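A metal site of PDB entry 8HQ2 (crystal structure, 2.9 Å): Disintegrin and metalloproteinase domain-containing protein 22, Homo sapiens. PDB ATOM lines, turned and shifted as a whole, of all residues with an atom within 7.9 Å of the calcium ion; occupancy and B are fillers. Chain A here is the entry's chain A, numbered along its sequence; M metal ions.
O of Glu 10 is in hydrogen-bond range of N of Asp 93 (2.8 Å). The backbone carbonyl oxygen of Asp 93 sits at hydrogen-bond distance from the backbone NH of Cys 117 (3.0 Å). SG of Cys 201 is disulfide-bonded to SG of Cys 117, at 2.0 Å. The backbone NH (N) of Ala 94 sits at hydrogen-bond distance from the backbone carbonyl oxygen (O) of Glu 10. The backbone carbonyl oxygen of Leu 202 sits at hydrogen-bond distance from the backbone NH of Tyr 8 (2.8 Å).
The calcium ion is bound by OD1 of Asn 204 (2.3 Å), OD2 of Asp 93 (2.5 Å), OD1 of Asp 93 (2.7 Å) and O of Cys 201 (2.8 Å).
O of Tyr 8 touches the calcium ion, 3.96 Å away. OE2 of Glu 10 touches the calcium ion, at 3.7 Å. Within 4 Å of the calcium ion: Tyr 8, Glu 10, Asp 93, Cys 201 and Asn 204.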
ATOM      1  N   LYS A   7      15.034   8.450  19.125  1.00  0.00           N
ATOM      2  CA  LYS A   7      15.118   9.631  18.270  1.00  0.00           C
ATOM      3  C   LYS A   7      13.719  10.108  17.913  1.00  0.00           C
ATOM      4  O   LYS A   7      12.816   9.297  17.697  1.00  0.00           O
ATOM      5  CB  LYS A   7      15.922   9.317  17.007  1.00  0.00           C
ATOM      6  CG  LYS A   7      17.400   9.162  17.281  1.00  0.00           C
ATOM      7  CD  LYS A   7      18.046   8.230  16.294  1.00  0.00           C
ATOM      8  CE  LYS A   7      17.581   6.782  16.494  1.00  0.00           C
ATOM      9  NZ  LYS A   7      18.259   6.113  17.638  1.00  0.00           N
ATOM     10  N   TYR A   8      13.535  11.423  17.900  1.00  0.00           N
ATOM     11  CA  TYR A   8      12.231  12.029  17.652  1.00  0.00           C
ATOM     12  C   TYR A   8      12.308  12.934  16.434  1.00  0.00           C
ATOM     13  O   TYR A   8      13.148  13.834  16.373  1.00  0.00           O
ATOM     14  CB  TYR A   8      11.775  12.820  18.883  1.00  0.00           C
ATOM     15  CG  TYR A   8      11.976  12.091  20.195  1.00  0.00           C
ATOM     16  CD1 TYR A   8      13.164  12.196  20.893  1.00  0.00           C
ATOM     17  CD2 TYR A   8      10.970  11.292  20.720  1.00  0.00           C
ATOM     18  CE1 TYR A   8      13.358  11.526  22.084  1.00  0.00           C
ATOM     19  CE2 TYR A   8      11.155  10.619  21.914  1.00  0.00           C
ATOM     20  CZ  TYR A   8      12.349  10.747  22.593  1.00  0.00           C
ATOM     21  OH  TYR A   8      12.533  10.073  23.787  1.00  0.00           O
ATOM     22  N   ILE A   9      11.408  12.703  15.480  1.00  0.00           N
ATOM     23  CA  ILE A   9      11.331  13.507  14.260  1.00  0.00           C
ATOM     24  C   ILE A   9      10.166  14.474  14.420  1.00  0.00           C
ATOM     25  O   ILE A   9       9.002  14.056  14.419  1.00  0.00           O
ATOM     26  CB  ILE A   9      11.158  12.634  13.013  1.00  0.00           C
ATOM     27  CG1 ILE A   9      12.374  11.743  12.805  1.00  0.00           C
ATOM     28  CG2 ILE A   9      10.912  13.499  11.793  1.00  0.00           C
ATOM     29  CD1 ILE A   9      12.267  10.863  11.594  1.00  0.00           C
ATOM     30  N   GLU A  10      10.460  15.766  14.541  1.00  0.00           N
ATOM     31  CA  GLU A  10       9.411  16.780  14.523  1.00  0.00           C
ATOM     32  C   GLU A  10       9.018  17.056  13.082  1.00  0.00           C
ATOM     33  O   GLU A  10       9.843  17.489  12.271  1.00  0.00           O
ATOM     34  CB  GLU A  10       9.874  18.052  15.216  1.00  0.00           C
ATOM     35  CG  GLU A  10      10.114  17.886  16.715  1.00  0.00           C
ATOM     36  CD  GLU A  10      10.380  19.206  17.409  1.00  0.00           C
ATOM     37  OE1 GLU A  10       9.698  19.503  18.414  1.00  0.00           O
ATOM     38  OE2 GLU A  10      11.270  19.954  16.945  1.00  0.00           O
ATOM     39  N   LEU A  11       7.748  16.837  12.765  1.00  0.00           N
ATOM     40  CA  LEU A  11       7.270  16.864  11.386  1.00  0.00           C
ATOM     41  C   LEU A  11       6.182  17.920  11.239  1.00  0.00           C
ATOM     42  O   LEU A  11       5.259  18.004  12.062  1.00  0.00           O
ATOM     43  CB  LEU A  11       6.734  15.490  10.971  1.00  0.00           C
ATOM     44  CG  LEU A  11       5.920  15.427   9.674  1.00  0.00           C
ATOM     45  CD1 LEU A  11       6.799  15.663   8.450  1.00  0.00           C
ATOM     46  CD2 LEU A  11       5.220  14.092   9.578  1.00  0.00           C
ATOM     47  N   SER A  92      10.740  22.909  12.746  1.00  0.00           N
ATOM     48  CA  SER A  92      10.483  21.491  12.552  1.00  0.00           C
ATOM     49  C   SER A  92      11.751  20.813  12.053  1.00  0.00           C
ATOM     50  O   SER A  92      12.624  21.444  11.454  1.00  0.00           O
ATOM     51  CB  SER A  92       9.332  21.265  11.564  1.00  0.00           C
ATOM     52  OG  SER A  92       9.714  21.704  10.267  1.00  0.00           O
ATOM     53  N   ASP A  93      11.829  19.509  12.301  1.00  0.00           N
ATOM     54  CA  ASP A  93      12.916  18.710  11.749  1.00  0.00           C
ATOM     55  C   ASP A  93      12.703  18.441  10.267  1.00  0.00           C
ATOM     56  O   ASP A  93      13.679  18.390   9.494  1.00  0.00           O
ATOM     57  CB  ASP A  93      13.033  17.393  12.518  1.00  0.00           C
ATOM     58  CG  ASP A  93      13.361  17.593  13.974  1.00  0.00           C
ATOM     59  OD1 ASP A  93      14.020  18.600  14.294  1.00  0.00           O
ATOM     60  OD2 ASP A  93      12.944  16.759  14.798  1.00  0.00           O
ATOM     61  N   ALA A  94      11.458  18.253   9.847  1.00  0.00           N
ATOM     62  CA  ALA A  94      11.144  17.956   8.457  1.00  0.00           C
ATOM     63  C   ALA A  94       9.788  18.545   8.100  1.00  0.00           C
ATOM     64  O   ALA A  94       8.864  18.547   8.914  1.00  0.00           O
ATOM     65  CB  ALA A  94      11.131  16.439   8.208  1.00  0.00           C
ATOM     66  N   ILE A 116      17.551  15.562   6.516  1.00  0.00           N
ATOM     67  CA  ILE A 116      16.796  15.849   7.729  1.00  0.00           C
ATOM     68  C   ILE A 116      17.412  17.045   8.452  1.00  0.00           C
ATOM     69  O   ILE A 116      18.630  17.168   8.574  1.00  0.00           O
ATOM     70  CB  ILE A 116      16.737  14.609   8.637  1.00  0.00           C
ATOM     71  CG1 ILE A 116      15.880  14.894   9.881  1.00  0.00           C
ATOM     72  CG2 ILE A 116      18.126  14.144   9.036  1.00  0.00           C
ATOM     73  CD1 ILE A 116      14.445  15.235   9.573  1.00  0.00           C
ATOM     74  N   CYS A 117      16.541  17.951   8.908  1.00  0.00           N
ATOM     75  CA  CYS A 117      16.893  19.143   9.668  1.00  0.00           C
ATOM     76  C   CYS A 117      17.745  20.123   8.889  1.00  0.00           C
ATOM     77  O   CYS A 117      18.463  20.935   9.474  1.00  0.00           O
ATOM     78  CB  CYS A 117      17.586  18.774  10.970  1.00  0.00           C
ATOM     79  SG  CYS A 117      16.495  17.918  12.066  1.00  0.00           S
ATOM     80  N   GLY A 199      21.508  14.203  11.343  1.00  0.00           N
ATOM     81  CA  GLY A 199      20.327  14.283  12.190  1.00  0.00           C
ATOM     82  C   GLY A 199      20.601  14.494  13.670  1.00  0.00           C
ATOM     83  O   GLY A 199      20.017  13.792  14.517  1.00  0.00           O
ATOM     84  N   ALA A 200      21.464  15.446  13.999  1.00  0.00           N
ATOM     85  CA  ALA A 200      21.736  15.746  15.401  1.00  0.00           C
ATOM     86  C   ALA A 200      20.483  16.267  16.101  1.00  0.00           C
ATOM     87  O   ALA A 200      20.219  15.938  17.267  1.00  0.00           O
ATOM     88  CB  ALA A 200      22.868  16.760  15.513  1.00  0.00           C
ATOM     89  N   CYS A 201      19.708  17.103  15.404  1.00  0.00           N
ATOM     90  CA  CYS A 201      18.434  17.609  15.899  1.00  0.00           C
ATOM     91  C   CYS A 201      17.514  16.516  16.427  1.00  0.00           C
ATOM     92  O   CYS A 201      16.772  16.742  17.383  1.00  0.00           O
ATOM     93  CB  CYS A 201      17.730  18.323  14.772  1.00  0.00           C
ATOM     94  SG  CYS A 201      17.800  17.184  13.398  1.00  0.00           S
ATOM     95  N   LEU A 202      17.524  15.343  15.793  1.00  0.00           N
ATOM     96  CA  LEU A 202      16.575  14.288  16.124  1.00  0.00           C
ATOM     97  C   LEU A 202      16.618  13.894  17.584  1.00  0.00           C
ATOM     98  O   LEU A 202      15.651  13.305  18.091  1.00  0.00           O
ATOM     99  CB  LEU A 202      16.833  13.053  15.261  1.00  0.00           C
ATOM    100  CG  LEU A 202      16.696  13.211  13.744  1.00  0.00           C
ATOM    101  CD1 LEU A 202      16.741  11.849  13.077  1.00  0.00           C
ATOM    102  CD2 LEU A 202      15.416  13.939  13.379  1.00  0.00           C
ATOM    103  N   PHE A 203      17.712  14.189  18.289  1.00  0.00           N
ATOM    104  CA  PHE A 203      17.849  13.812  19.684  1.00  0.00           C
ATOM    105  C   PHE A 203      17.181  14.806  20.628  1.00  0.00           C
ATOM    106  O   PHE A 203      17.048  14.502  21.823  1.00  0.00           O
ATOM    107  CB  PHE A 203      19.339  13.660  20.018  1.00  0.00           C
ATOM    108  CG  PHE A 203      20.037  12.676  19.127  1.00  0.00           C
ATOM    109  CD1 PHE A 203      20.101  11.332  19.465  1.00  0.00           C
ATOM    110  CD2 PHE A 203      20.610  13.078  17.936  1.00  0.00           C
ATOM    111  CE1 PHE A 203      20.736  10.427  18.646  1.00  0.00           C
ATOM    112  CE2 PHE A 203      21.241  12.170  17.107  1.00  0.00           C
ATOM    113  CZ  PHE A 203      21.302  10.849  17.462  1.00  0.00           C
ATOM    114  N   ASN A 204      16.766  15.962  20.123  1.00  0.00           N
ATOM    115  CA  ASN A 204      15.922  16.859  20.910  1.00  0.00           C
ATOM    116  C   ASN A 204      14.524  16.272  21.037  1.00  0.00           C
ATOM    117  O   ASN A 204      13.954  15.746  20.079  1.00  0.00           O
ATOM    118  CB  ASN A 204      15.866  18.242  20.244  1.00  0.00           C
ATOM    119  CG  ASN A 204      14.443  18.708  19.984  1.00  0.00           C
ATOM    120  OD1 ASN A 204      13.843  18.372  18.961  1.00  0.00           O
ATOM    121  ND2 ASN A 204      13.892  19.500  20.908  1.00  0.00           N
ATOM    122  N   LYS A 205      13.962  16.363  22.248  1.00  0.00           N
ATOM    123  CA  LYS A 205      12.636  15.832  22.521  1.00  0.00           C
ATOM    124  C   LYS A 205      11.595  16.938  22.400  1.00  0.00           C
ATOM    125  O   LYS A 205      11.813  18.032  22.934  1.00  0.00           O
ATOM    126  CB  LYS A 205      12.581  15.222  23.909  1.00  0.00           C
ATOM    127  CG  LYS A 205      11.407  14.302  24.161  1.00  0.00           C
ATOM    128  CD  LYS A 205      11.546  13.627  25.520  1.00  0.00           C
ATOM    129  CE  LYS A 205      10.437  12.630  25.785  1.00  0.00           C
ATOM    130  NZ  LYS A 205      10.534  12.060  27.160  1.00  0.00           N
ATOM    131  N   PRO A 206      10.488  16.705  21.703  1.00  0.00           N
ATOM    132  CA  PRO A 206       9.540  17.791  21.419  1.00  0.00           C
ATOM    133  C   PRO A 206       8.887  18.329  22.693  1.00  0.00           C
ATOM    134  O   PRO A 206       8.396  17.560  23.521  1.00  0.00           O
ATOM    135  CB  PRO A 206       8.504  17.135  20.496  1.00  0.00           C
ATOM    136  CG  PRO A 206       9.213  15.950  19.917  1.00  0.00           C
ATOM    137  CD  PRO A 206      10.114  15.466  21.007  1.00  0.00           C
HETATM  138 CA    CA M   1      14.194  17.630  16.786  1.00  0.00          CA
